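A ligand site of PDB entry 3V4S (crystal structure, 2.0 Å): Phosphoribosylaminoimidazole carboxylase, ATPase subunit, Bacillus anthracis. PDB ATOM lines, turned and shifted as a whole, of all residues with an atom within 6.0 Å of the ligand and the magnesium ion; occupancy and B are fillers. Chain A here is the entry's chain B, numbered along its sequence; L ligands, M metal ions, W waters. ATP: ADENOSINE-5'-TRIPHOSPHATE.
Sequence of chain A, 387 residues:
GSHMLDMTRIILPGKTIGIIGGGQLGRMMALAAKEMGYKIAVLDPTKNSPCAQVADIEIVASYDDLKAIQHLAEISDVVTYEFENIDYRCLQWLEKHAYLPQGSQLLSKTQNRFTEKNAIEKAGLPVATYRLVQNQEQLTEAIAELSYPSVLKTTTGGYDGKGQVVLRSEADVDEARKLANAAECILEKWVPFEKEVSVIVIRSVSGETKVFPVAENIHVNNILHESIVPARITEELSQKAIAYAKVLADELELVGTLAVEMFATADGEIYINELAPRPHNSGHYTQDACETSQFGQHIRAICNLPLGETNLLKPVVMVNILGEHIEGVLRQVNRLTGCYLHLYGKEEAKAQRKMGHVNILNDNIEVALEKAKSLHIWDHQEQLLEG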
ATOM      1  N   ARG A 113      11.866 -29.966 -21.899  1.00  0.00           N
ATOM      2  CA  ARG A 113      12.856 -29.854 -20.823  1.00  0.00           C
ATOM      3  C   ARG A 113      12.228 -29.897 -19.442  1.00  0.00           C
ATOM      4  O   ARG A 113      12.825 -30.437 -18.505  1.00  0.00           O
ATOM      5  CB  ARG A 113      13.675 -28.572 -20.963  1.00  0.00           C
ATOM      6  CG  ARG A 113      14.557 -28.496 -22.178  1.00  0.00           C
ATOM      7  CD  ARG A 113      15.527 -27.338 -22.031  1.00  0.00           C
ATOM      8  NE  ARG A 113      16.271 -27.076 -23.251  1.00  0.00           N
ATOM      9  CZ  ARG A 113      17.384 -27.723 -23.608  1.00  0.00           C
ATOM     10  NH1 ARG A 113      17.892 -28.660 -22.816  1.00  0.00           N
ATOM     11  NH2 ARG A 113      17.991 -27.412 -24.749  1.00  0.00           N
ATOM     12  N   ALA A 128      20.076 -29.586 -12.121  1.00  0.00           N
ATOM     13  CA  ALA A 128      20.183 -28.189 -11.762  1.00  0.00           C
ATOM     14  C   ALA A 128      18.790 -27.696 -11.328  1.00  0.00           C
ATOM     15  O   ALA A 128      17.784 -28.056 -11.957  1.00  0.00           O
ATOM     16  CB  ALA A 128      20.720 -27.372 -12.922  1.00  0.00           C
ATOM     17  N   VAL A 151      20.798 -20.104 -16.336  1.00  0.00           N
ATOM     18  CA  VAL A 151      20.668 -20.280 -17.758  1.00  0.00           C
ATOM     19  C   VAL A 151      19.199 -20.479 -18.092  1.00  0.00           C
ATOM     20  O   VAL A 151      18.533 -21.321 -17.505  1.00  0.00           O
ATOM     21  CB  VAL A 151      21.493 -21.478 -18.284  1.00  0.00           C
ATOM     22  CG1 VAL A 151      21.241 -21.703 -19.769  1.00  0.00           C
ATOM     23  CG2 VAL A 151      22.987 -21.230 -18.053  1.00  0.00           C
ATOM     24  N   LYS A 153      16.498 -21.643 -20.926  1.00  0.00           N
ATOM     25  CA  LYS A 153      16.447 -22.570 -22.059  1.00  0.00           C
ATOM     26  C   LYS A 153      15.004 -22.740 -22.482  1.00  0.00           C
ATOM     27  O   LYS A 153      14.149 -22.967 -21.624  1.00  0.00           O
ATOM     28  CB  LYS A 153      16.959 -23.962 -21.650  1.00  0.00           C
ATOM     29  CG  LYS A 153      18.344 -24.035 -21.012  1.00  0.00           C
ATOM     30  CD  LYS A 153      18.747 -25.501 -20.772  1.00  0.00           C
ATOM     31  CE  LYS A 153      20.204 -25.551 -20.305  1.00  0.00           C
ATOM     32  NZ  LYS A 153      20.656 -26.940 -19.979  1.00  0.00           N
ATOM     33  N   GLY A 158      15.073 -26.844 -28.816  1.00  0.00           N
ATOM     34  CA  GLY A 158      16.461 -26.415 -28.617  1.00  0.00           C
ATOM     35  C   GLY A 158      17.483 -27.455 -29.061  1.00  0.00           C
ATOM     36  O   GLY A 158      17.301 -28.652 -28.825  1.00  0.00           O
ATOM     37  N   TYR A 159      18.536 -27.000 -29.734  1.00  0.00           N
ATOM     38  CA  TYR A 159      19.676 -27.838 -30.117  1.00  0.00           C
ATOM     39  C   TYR A 159      20.835 -26.894 -30.370  1.00  0.00           C
ATOM     40  O   TYR A 159      20.636 -25.733 -30.748  1.00  0.00           O
ATOM     41  CB  TYR A 159      19.389 -28.689 -31.377  1.00  0.00           C
ATOM     42  CG  TYR A 159      19.100 -27.851 -32.606  1.00  0.00           C
ATOM     43  CD1 TYR A 159      17.808 -27.352 -32.840  1.00  0.00           C
ATOM     44  CD2 TYR A 159      20.104 -27.546 -33.526  1.00  0.00           C
ATOM     45  CE1 TYR A 159      17.527 -26.565 -33.949  1.00  0.00           C
ATOM     46  CE2 TYR A 159      19.827 -26.759 -34.648  1.00  0.00           C
ATOM     47  CZ  TYR A 159      18.545 -26.277 -34.850  1.00  0.00           C
ATOM     48  OH  TYR A 159      18.262 -25.500 -35.944  1.00  0.00           O
ATOM     49  N   ASP A 160      22.060 -27.386 -30.147  1.00  0.00           N
ATOM     50  CA  ASP A 160      23.272 -26.580 -30.347  1.00  0.00           C
ATOM     51  C   ASP A 160      23.247 -25.243 -29.570  1.00  0.00           C
ATOM     52  O   ASP A 160      23.827 -24.244 -30.000  1.00  0.00           O
ATOM     53  CB  ASP A 160      23.519 -26.358 -31.852  1.00  0.00           C
ATOM     54  CG  ASP A 160      23.954 -27.627 -32.567  1.00  0.00           C
ATOM     55  OD1 ASP A 160      24.260 -28.645 -31.904  1.00  0.00           O
ATOM     56  OD2 ASP A 160      23.982 -27.625 -33.807  1.00  0.00           O
ATOM     57  N   GLY A 161      22.567 -25.250 -28.408  1.00  0.00           N
ATOM     58  CA  GLY A 161      22.408 -24.049 -27.579  1.00  0.00           C
ATOM     59  C   GLY A 161      21.512 -22.952 -28.151  1.00  0.00           C
ATOM     60  O   GLY A 161      21.472 -21.838 -27.603  1.00  0.00           O
ATOM     61  N   LYS A 162      20.803 -23.242 -29.234  1.00  0.00           N
ATOM     62  CA  LYS A 162      19.819 -22.293 -29.777  1.00  0.00           C
ATOM     63  C   LYS A 162      18.623 -22.227 -28.842  1.00  0.00           C
ATOM     64  O   LYS A 162      18.149 -23.261 -28.360  1.00  0.00           O
ATOM     65  CB  LYS A 162      19.361 -22.698 -31.185  1.00  0.00           C
ATOM     66  CG  LYS A 162      20.420 -22.506 -32.265  1.00  0.00           C
ATOM     67  CD  LYS A 162      19.880 -22.964 -33.607  1.00  0.00           C
ATOM     68  CE  LYS A 162      20.974 -23.120 -34.643  1.00  0.00           C
ATOM     69  NZ  LYS A 162      21.670 -21.844 -34.956  1.00  0.00           N
ATOM     70  N   GLN A 164      18.887 -20.439 -25.948  1.00  0.00           N
ATOM     71  CA  GLN A 164      19.511 -20.365 -24.629  1.00  0.00           C
ATOM     72  C   GLN A 164      20.124 -19.004 -24.357  1.00  0.00           C
ATOM     73  O   GLN A 164      20.695 -18.397 -25.255  1.00  0.00           O
ATOM     74  CB  GLN A 164      20.583 -21.423 -24.449  1.00  0.00           C
ATOM     75  CG  GLN A 164      19.995 -22.811 -24.303  1.00  0.00           C
ATOM     76  CD  GLN A 164      20.948 -23.812 -23.687  1.00  0.00           C
ATOM     77  OE1 GLN A 164      22.017 -23.465 -23.136  1.00  0.00           O
ATOM     78  NE2 GLN A 164      20.556 -25.094 -23.759  1.00  0.00           N
ATOM     79  N   GLU A 188      17.288 -22.377 -15.057  1.00  0.00           N
ATOM     80  CA  GLU A 188      17.962 -23.292 -14.153  1.00  0.00           C
ATOM     81  C   GLU A 188      19.292 -22.724 -13.693  1.00  0.00           C
ATOM     82  O   GLU A 188      19.940 -21.946 -14.410  1.00  0.00           O
ATOM     83  CB  GLU A 188      18.157 -24.669 -14.809  1.00  0.00           C
ATOM     84  CG  GLU A 188      19.122 -24.676 -15.985  1.00  0.00           C
ATOM     85  CD  GLU A 188      19.328 -26.067 -16.587  1.00  0.00           C
ATOM     86  OE1 GLU A 188      18.399 -26.897 -16.550  1.00  0.00           O
ATOM     87  OE2 GLU A 188      20.419 -26.291 -17.123  1.00  0.00           O
ATOM     88  N   LYS A 189      19.695 -23.111 -12.481  1.00  0.00           N
ATOM     89  CA  LYS A 189      20.983 -22.699 -11.936  1.00  0.00           C
ATOM     90  C   LYS A 189      22.138 -23.158 -12.811  1.00  0.00           C
ATOM     91  O   LYS A 189      22.109 -24.258 -13.394  1.00  0.00           O
ATOM     92  CB  LYS A 189      21.156 -23.242 -10.523  1.00  0.00           C
ATOM     93  CG  LYS A 189      20.312 -22.514  -9.497  1.00  0.00           C
ATOM     94  CD  LYS A 189      20.570 -23.029  -8.089  1.00  0.00           C
ATOM     95  CE  LYS A 189      19.692 -22.309  -7.066  1.00  0.00           C
ATOM     96  NZ  LYS A 189      19.785 -22.954  -5.718  1.00  0.00           N
ATOM     97  N   TRP A 190      23.141 -22.288 -12.931  1.00  0.00           N
ATOM     98  CA  TRP A 190      24.424 -22.640 -13.516  1.00  0.00           C
ATOM     99  C   TRP A 190      25.096 -23.703 -12.676  1.00  0.00           C
ATOM    100  O   TRP A 190      25.070 -23.644 -11.436  1.00  0.00           O
ATOM    101  CB  TRP A 190      25.289 -21.404 -13.568  1.00  0.00           C
ATOM    102  CG  TRP A 190      26.654 -21.628 -14.175  1.00  0.00           C
ATOM    103  CD1 TRP A 190      27.845 -21.881 -13.501  1.00  0.00           C
ATOM    104  CD2 TRP A 190      27.009 -21.623 -15.596  1.00  0.00           C
ATOM    105  NE1 TRP A 190      28.884 -22.038 -14.391  1.00  0.00           N
ATOM    106  CE2 TRP A 190      28.451 -21.886 -15.659  1.00  0.00           C
ATOM    107  CE3 TRP A 190      26.310 -21.437 -16.770  1.00  0.00           C
ATOM    108  CZ2 TRP A 190      29.129 -21.954 -16.864  1.00  0.00           C
ATOM    109  CZ3 TRP A 190      26.997 -21.503 -17.979  1.00  0.00           C
ATOM    110  CH2 TRP A 190      28.378 -21.757 -18.024  1.00  0.00           C
ATOM    111  N   VAL A 191      25.668 -24.706 -13.341  1.00  0.00           N
ATOM    112  CA  VAL A 191      26.405 -25.746 -12.646  1.00  0.00           C
ATOM    113  C   VAL A 191      27.891 -25.546 -12.945  1.00  0.00           C
ATOM    114  O   VAL A 191      28.297 -25.585 -14.109  1.00  0.00           O
ATOM    115  CB  VAL A 191      25.928 -27.159 -13.041  1.00  0.00           C
ATOM    116  CG1 VAL A 191      26.744 -28.222 -12.315  1.00  0.00           C
ATOM    117  CG2 VAL A 191      24.445 -27.327 -12.726  1.00  0.00           C
ATOM    118  N   PRO A 192      28.709 -25.288 -11.905  1.00  0.00           N
ATOM    119  CA  PRO A 192      30.122 -25.049 -12.159  1.00  0.00           C
ATOM    120  C   PRO A 192      30.918 -26.367 -12.266  1.00  0.00           C
ATOM    121  O   PRO A 192      31.852 -26.575 -11.518  1.00  0.00           O
ATOM    122  CB  PRO A 192      30.560 -24.230 -10.930  1.00  0.00           C
ATOM    123  CG  PRO A 192      29.641 -24.679  -9.823  1.00  0.00           C
ATOM    124  CD  PRO A 192      28.395 -25.263 -10.465  1.00  0.00           C
ATOM    125  N   PHE A 193      30.555 -27.213 -13.231  1.00  0.00           N
ATOM    126  CA  PHE A 193      31.168 -28.532 -13.410  1.00  0.00           C
ATOM    127  C   PHE A 193      32.665 -28.506 -13.742  1.00  0.00           C
ATOM    128  O   PHE A 193      33.189 -27.504 -14.246  1.00  0.00           O
ATOM    129  CB  PHE A 193      30.409 -29.323 -14.479  1.00  0.00           C
ATOM    130  CG  PHE A 193      30.367 -28.658 -15.836  1.00  0.00           C
ATOM    131  CD1 PHE A 193      29.226 -27.989 -16.265  1.00  0.00           C
ATOM    132  CD2 PHE A 193      31.469 -28.686 -16.680  1.00  0.00           C
ATOM    133  CE1 PHE A 193      29.178 -27.378 -17.505  1.00  0.00           C
ATOM    134  CE2 PHE A 193      31.439 -28.073 -17.929  1.00  0.00           C
ATOM    135  CZ  PHE A 193      30.276 -27.427 -18.343  1.00  0.00           C
ATOM    136  N   GLU A 196      32.128 -32.228 -18.517  1.00  0.00           N
ATOM    137  CA  GLU A 196      30.872 -32.783 -19.008  1.00  0.00           C
ATOM    138  C   GLU A 196      31.130 -34.195 -19.484  1.00  0.00           C
ATOM    139  O   GLU A 196      32.130 -34.457 -20.148  1.00  0.00           O
ATOM    140  CB  GLU A 196      30.367 -32.008 -20.222  1.00  0.00           C
ATOM    141  CG  GLU A 196      30.094 -30.543 -19.979  1.00  0.00           C
ATOM    142  CD  GLU A 196      29.314 -29.942 -21.114  1.00  0.00           C
ATOM    143  OE1 GLU A 196      29.886 -29.076 -21.817  1.00  0.00           O
ATOM    144  OE2 GLU A 196      28.151 -30.356 -21.324  1.00  0.00           O
ATOM    145  N   HIS A 219      32.424 -29.069 -25.653  1.00  0.00           N
ATOM    146  CA  HIS A 219      31.537 -28.306 -26.504  1.00  0.00           C
ATOM    147  C   HIS A 219      32.197 -26.986 -26.806  1.00  0.00           C
ATOM    148  O   HIS A 219      32.936 -26.460 -25.967  1.00  0.00           O
ATOM    149  CB  HIS A 219      30.208 -28.077 -25.792  1.00  0.00           C
ATOM    150  CG  HIS A 219      29.394 -29.325 -25.615  1.00  0.00           C
ATOM    151  ND1 HIS A 219      29.438 -30.068 -24.500  1.00  0.00           N
ATOM    152  CD2 HIS A 219      28.507 -29.964 -26.479  1.00  0.00           C
ATOM    153  CE1 HIS A 219      28.595 -31.117 -24.620  1.00  0.00           C
ATOM    154  NE2 HIS A 219      28.031 -31.050 -25.836  1.00  0.00           N
ATOM    155  N   ASN A 222      28.432 -24.127 -27.944  1.00  0.00           N
ATOM    156  CA  ASN A 222      27.322 -25.068 -27.625  1.00  0.00           C
ATOM    157  C   ASN A 222      27.124 -26.239 -28.599  1.00  0.00           C
ATOM    158  O   ASN A 222      26.062 -26.883 -28.580  1.00  0.00           O
ATOM    159  CB  ASN A 222      25.998 -24.313 -27.461  1.00  0.00           C
ATOM    160  CG  ASN A 222      26.012 -23.390 -26.272  1.00  0.00           C
ATOM    161  OD1 ASN A 222      25.582 -22.225 -26.362  1.00  0.00           O
ATOM    162  ND2 ASN A 222      26.526 -23.872 -25.138  1.00  0.00           N
ATOM    163  N   ILE A 223      28.117 -26.495 -29.457  1.00  0.00           N
ATOM    164  CA  ILE A 223      28.073 -27.640 -30.358  1.00  0.00           C
ATOM    165  C   ILE A 223      29.179 -28.592 -29.928  1.00  0.00           C
ATOM    166  O   ILE A 223      30.279 -28.153 -29.619  1.00  0.00           O
ATOM    167  CB  ILE A 223      28.321 -27.230 -31.829  1.00  0.00           C
ATOM    168  CG1 ILE A 223      27.364 -26.104 -32.256  1.00  0.00           C
ATOM    169  CG2 ILE A 223      28.166 -28.441 -32.761  1.00  0.00           C
ATOM    170  CD1 ILE A 223      27.673 -25.511 -33.609  1.00  0.00           C
ATOM    171  N   GLU A 261      23.445 -37.001 -20.885  1.00  0.00           N
ATOM    172  CA  GLU A 261      24.464 -35.963 -20.708  1.00  0.00           C
ATOM    173  C   GLU A 261      24.518 -35.534 -19.244  1.00  0.00           C
ATOM    174  O   GLU A 261      23.468 -35.306 -18.615  1.00  0.00           O
ATOM    175  CB  GLU A 261      24.149 -34.725 -21.545  1.00  0.00           C
ATOM    176  CG  GLU A 261      24.131 -34.934 -23.046  1.00  0.00           C
ATOM    177  CD  GLU A 261      23.927 -33.626 -23.794  1.00  0.00           C
ATOM    178  OE1 GLU A 261      23.955 -32.515 -23.190  1.00  0.00           O
ATOM    179  OE2 GLU A 261      23.736 -33.687 -25.007  1.00  0.00           O
ATOM    180  N   PHE A 263      26.896 -33.438 -15.881  1.00  0.00           N
ATOM    181  CA  PHE A 263      27.857 -32.445 -15.434  1.00  0.00           C
ATOM    182  C   PHE A 263      28.561 -33.036 -14.224  1.00  0.00           C
ATOM    183  O   PHE A 263      27.904 -33.474 -13.286  1.00  0.00           O
ATOM    184  CB  PHE A 263      27.171 -31.135 -15.039  1.00  0.00           C
ATOM    185  CG  PHE A 263      26.514 -30.397 -16.186  1.00  0.00           C
ATOM    186  CD1 PHE A 263      25.342 -29.680 -15.972  1.00  0.00           C
ATOM    187  CD2 PHE A 263      27.070 -30.402 -17.462  1.00  0.00           C
ATOM    188  CE1 PHE A 263      24.733 -28.976 -17.024  1.00  0.00           C
ATOM    189  CE2 PHE A 263      26.455 -29.710 -18.509  1.00  0.00           C
ATOM    190  CZ  PHE A 263      25.288 -28.991 -18.286  1.00  0.00           C
ATOM    191  N   ASN A 273      22.075 -33.353 -17.185  1.00  0.00           N
ATOM    192  CA  ASN A 273      21.800 -32.165 -17.988  1.00  0.00           C
ATOM    193  C   ASN A 273      20.590 -32.382 -18.889  1.00  0.00           C
ATOM    194  O   ASN A 273      19.662 -31.559 -18.909  1.00  0.00           O
ATOM    195  CB  ASN A 273      23.033 -31.735 -18.802  1.00  0.00           C
ATOM    196  CG  ASN A 273      22.732 -30.574 -19.759  1.00  0.00           C
ATOM    197  OD1 ASN A 273      22.186 -29.553 -19.366  1.00  0.00           O
ATOM    198  ND2 ASN A 273      23.153 -30.717 -21.005  1.00  0.00           N
ATOM    199  N   GLU A 274      20.627 -33.480 -19.659  1.00  0.00           N
ATOM    200  CA  GLU A 274      19.529 -33.828 -20.563  1.00  0.00           C
ATOM    201  C   GLU A 274      19.659 -35.221 -21.134  1.00  0.00           C
ATOM    202  O   GLU A 274      20.726 -35.841 -21.101  1.00  0.00           O
ATOM    203  CB  GLU A 274      19.370 -32.792 -21.692  1.00  0.00           C
ATOM    204  CG  GLU A 274      20.488 -32.789 -22.723  1.00  0.00           C
ATOM    205  CD  GLU A 274      20.241 -31.846 -23.891  1.00  0.00           C
ATOM    206  OE1 GLU A 274      21.175 -31.661 -24.704  1.00  0.00           O
ATOM    207  OE2 GLU A 274      19.105 -31.298 -24.023  1.00  0.00           O
ATOM    208  N   ARG A 278      17.861 -41.747 -28.452  1.00  0.00           N
ATOM    209  CA  ARG A 278      18.389 -42.119 -29.762  1.00  0.00           C
ATOM    210  C   ARG A 278      19.917 -42.169 -29.657  1.00  0.00           C
ATOM    211  O   ARG A 278      20.509 -41.604 -28.698  1.00  0.00           O
ATOM    212  CB  ARG A 278      17.983 -41.056 -30.805  1.00  0.00           C
ATOM    213  CG  ARG A 278      18.314 -39.628 -30.356  1.00  0.00           C
ATOM    214  CD  ARG A 278      18.377 -38.597 -31.467  1.00  0.00           C
ATOM    215  NE  ARG A 278      18.613 -37.264 -30.925  1.00  0.00           N
ATOM    216  CZ  ARG A 278      19.810 -36.765 -30.633  1.00  0.00           C
ATOM    217  NH1 ARG A 278      20.925 -37.473 -30.842  1.00  0.00           N
ATOM    218  NH2 ARG A 278      19.898 -35.546 -30.117  1.00  0.00           N
ATOM    219  N   HIS A 280      23.518 -40.798 -30.188  1.00  0.00           N
ATOM    220  CA  HIS A 280      23.865 -39.428 -29.887  1.00  0.00           C
ATOM    221  C   HIS A 280      25.237 -39.186 -30.431  1.00  0.00           C
ATOM    222  O   HIS A 280      26.053 -40.109 -30.494  1.00  0.00           O
ATOM    223  CB  HIS A 280      23.893 -39.287 -28.368  1.00  0.00           C
ATOM    224  CG  HIS A 280      23.996 -37.871 -27.872  1.00  0.00           C
ATOM    225  ND1 HIS A 280      25.157 -37.342 -27.473  1.00  0.00           N
ATOM    226  CD2 HIS A 280      23.026 -36.889 -27.677  1.00  0.00           C
ATOM    227  CE1 HIS A 280      24.954 -36.066 -27.061  1.00  0.00           C
ATOM    228  NE2 HIS A 280      23.642 -35.798 -27.173  1.00  0.00           N
ATOM    229  N   LYS A 354      26.502 -30.401 -39.083  1.00  0.00           N
ATOM    230  CA  LYS A 354      27.332 -31.587 -38.851  1.00  0.00           C
ATOM    231  C   LYS A 354      27.411 -32.387 -40.149  1.00  0.00           C
ATOM    232  O   LYS A 354      26.412 -32.918 -40.612  1.00  0.00           O
ATOM    233  CB  LYS A 354      26.750 -32.436 -37.719  1.00  0.00           C
ATOM    234  CG  LYS A 354      26.791 -31.741 -36.365  1.00  0.00           C
ATOM    235  CD  LYS A 354      26.075 -32.507 -35.278  1.00  0.00           C
ATOM    236  CE  LYS A 354      26.121 -31.731 -33.953  1.00  0.00           C
ATOM    237  NZ  LYS A 354      25.518 -32.503 -32.834  1.00  0.00           N
HETATM  238  PG  ATP L   1      22.224 -30.323 -27.834  1.00  0.00           P
HETATM  239  O1G ATP L   1      23.019 -31.369 -27.100  1.00  0.00           O
HETATM  240  O2G ATP L   1      22.823 -29.841 -29.141  1.00  0.00           O
HETATM  241  O3G ATP L   1      20.765 -30.636 -27.922  1.00  0.00           O
HETATM  242  PB  ATP L   1      21.139 -28.115 -26.284  1.00  0.00           P
HETATM  243  O1B ATP L   1      20.787 -27.093 -27.327  1.00  0.00           O
HETATM  244  O2B ATP L   1      20.065 -28.934 -25.649  1.00  0.00           O
HETATM  245  O3B ATP L   1      22.373 -29.037 -26.831  1.00  0.00           O
HETATM  246  PA  ATP L   1      22.236 -27.985 -23.629  1.00  0.00           P
HETATM  247  O1A ATP L   1      22.754 -29.389 -23.857  1.00  0.00           O
HETATM  248  O2A ATP L   1      21.179 -27.740 -22.584  1.00  0.00           O
HETATM  249  O3A ATP L   1      21.800 -27.312 -25.037  1.00  0.00           O
HETATM  250  O5' ATP L   1      23.490 -27.053 -23.298  1.00  0.00           O
HETATM  251  C5' ATP L   1      24.553 -26.952 -24.235  1.00  0.00           C
HETATM  252  C4' ATP L   1      25.809 -26.711 -23.410  1.00  0.00           C
HETATM  253  O4' ATP L   1      25.659 -25.520 -22.607  1.00  0.00           O
HETATM  254  C3' ATP L   1      26.063 -27.828 -22.401  1.00  0.00           C
HETATM  255  O3' ATP L   1      26.690 -29.007 -22.960  1.00  0.00           O
HETATM  256  C2' ATP L   1      26.875 -27.098 -21.338  1.00  0.00           C
HETATM  257  O2' ATP L   1      28.257 -27.017 -21.709  1.00  0.00           O
HETATM  258  C1' ATP L   1      26.259 -25.699 -21.322  1.00  0.00           C
HETATM  259  N9  ATP L   1      25.240 -25.658 -20.248  1.00  0.00           N
HETATM  260  C8  ATP L   1      23.914 -25.897 -20.388  1.00  0.00           C
HETATM  261  N7  ATP L   1      23.272 -25.812 -19.196  1.00  0.00           N
HETATM  262  C5  ATP L   1      24.198 -25.508 -18.258  1.00  0.00           C
HETATM  263  C6  ATP L   1      24.216 -25.260 -16.787  1.00  0.00           C
HETATM  264  N6  ATP L   1      23.079 -25.317 -16.047  1.00  0.00           N
HETATM  265  N1  ATP L   1      25.411 -24.967 -16.215  1.00  0.00           N
HETATM  266  C2  ATP L   1      26.557 -24.895 -16.916  1.00  0.00           C
HETATM  267  N3  ATP L   1      26.611 -25.118 -18.235  1.00  0.00           N
HETATM  268  C4  ATP L   1      25.493 -25.405 -18.954  1.00  0.00           C
HETATM  269 MG    MG M   1      23.343 -31.089 -24.891  1.00  0.00          MG
HETATM  270  O   HOH W   1      19.224 -25.163 -26.619  1.00  0.00           O
HETATM  271  O   HOH W   2      25.371 -29.379 -27.737  1.00  0.00           O
HETATM  272  O   HOH W   3      22.467 -31.630 -31.186  1.00  0.00           O
HETATM  273  O   HOH W   4      25.204 -30.501 -25.119  1.00  0.00           O
HETATM  274  O   HOH W   5      26.413 -22.611 -22.681  1.00  0.00           O
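O3' of the ligand is in hydrogen-bond range of OE2 of Glu 196 (2.6 Å). The guanidinium group of Arg 113 lies within salt-bridge range of an oxygen (O2B) of the ligand (2.7 Å). O2G of the ligand sits at hydrogen-bond distance from N of Asp 160. NZ of Lys 153 is in salt-bridge range of O2A of the ligand (2.8 Å). The backbone NH (N) of Gly 161 lies within hydrogen-bond range of an oxygen (O1B) of the ligand (2.8 Å). The side-chain amide nitrogen (NE2) of Gln 164 is in hydrogen-bond range of an oxygen (O3A) of the ligand. N1 of the ligand sits at hydrogen-bond distance from N of Val 191. A nitrogen (N6) of the ligand is in hydrogen-bond range of the backbone carbonyl oxygen (O) of Lys 189, at 3.0 Å. OE2 of Glu 188 sits at hydrogen-bond distance from N6 of the ligand, at 3.0 Å. O1B of the ligand sits close to N of Tyr 159 (3.3 Å). ND2 of Asn 222 is in hydrogen-bond range of O4' of the ligand. The side-chain amide nitrogen (ND2) of Asn 273 lies close to an oxygen (O1A) of the ligand (3.2 Å). An oxygen (O3') of the ligand lies close to a ring nitrogen (ND1) of His 219 (3.3 Å).
The side-chain carboxylate (OE2) of Glu 274 lies within salt-bridge range of the guanidinium group (NH1) of Arg 113 (3.1 Å). The backbone carbonyl oxygen of Glu 261 lies within hydrogen-bond range of the backbone NH of Asn 273. OE2 of Glu 261 lies within hydrogen-bond range of NE2 of His 280, 3.0 Å away. ND1 of His 219 lies within hydrogen-bond range of OE1 of Glu 196, at 2.9 Å. The side-chain amino group of Lys 153 lies within salt-bridge range of the side-chain carboxylate of Glu 188, at 2.9 Å. The side-chain amino group (NZ) of Lys 153 lies within hydrogen-bond range of the side-chain amide oxygen (OD1) of Asn 273 (3.1 Å). The backbone carbonyl oxygen of Glu 188 sits at hydrogen-bond distance from the backbone NH of Val 151, 2.8 Å away.
Gly 158 touches the ligand (C to O1B, 3.7 Å). Trp 190 touches the ligand (CE3 to C2, 3.5 Å). CE1 of Phe 193 touches N3 of the ligand, at 3.5 Å. Phe 263 touches the ligand (CZ to C5, 3.6 Å). Hydrophobic or aromatic side chains within 4 Å of the ligand: Trp 190, Val 191, Phe 193, His 219 and Phe 263. Of the 27 residues printed, 19 come within 4 Å of the ligand.
Asn 273 touches the magnesium ion. Within 4 Å of the magnesium ion: Glu 261, Asn 273 and Glu 274. The nearest printed residue that does not touch the magnesium ion is His 219 (4.8 Å).
The magnesium ion is bound by water W4, 2.0 Å away. An oxygen (O1A) of the ligand binds the magnesium ion (2.1 Å). The magnesium ion is bound by OE1 of Glu 274, 2.2 Å away. O1G of the ligand binds the magnesium ion (2.3 Å). OE1 of Glu 261 binds the magnesium ion. Slightly farther from the magnesium ion lies OE2 of Glu 261 (2.6 Å).
Water W4 bridges NE2 of His 219 (3.0 Å) and O3' of the ligand (3.0 Å). Water W1 lies within hydrogen-bond range of an oxygen (O1B) of the ligand (2.6 Å), the backbone carbonyl oxygen (O) of Lys 162 (2.8 Å), the side-chain amide nitrogen (NE2) of Gln 164 (3.2 Å) and the guanidinium group (NH2) of Arg 113 (3.2 Å). Water W2 bridges O of Asn 222 and O2G of the ligand. Water W5 lies within hydrogen-bond range of ND2 of Asn 222 (2.8 Å) and O4' of the ligand (3.0 Å).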
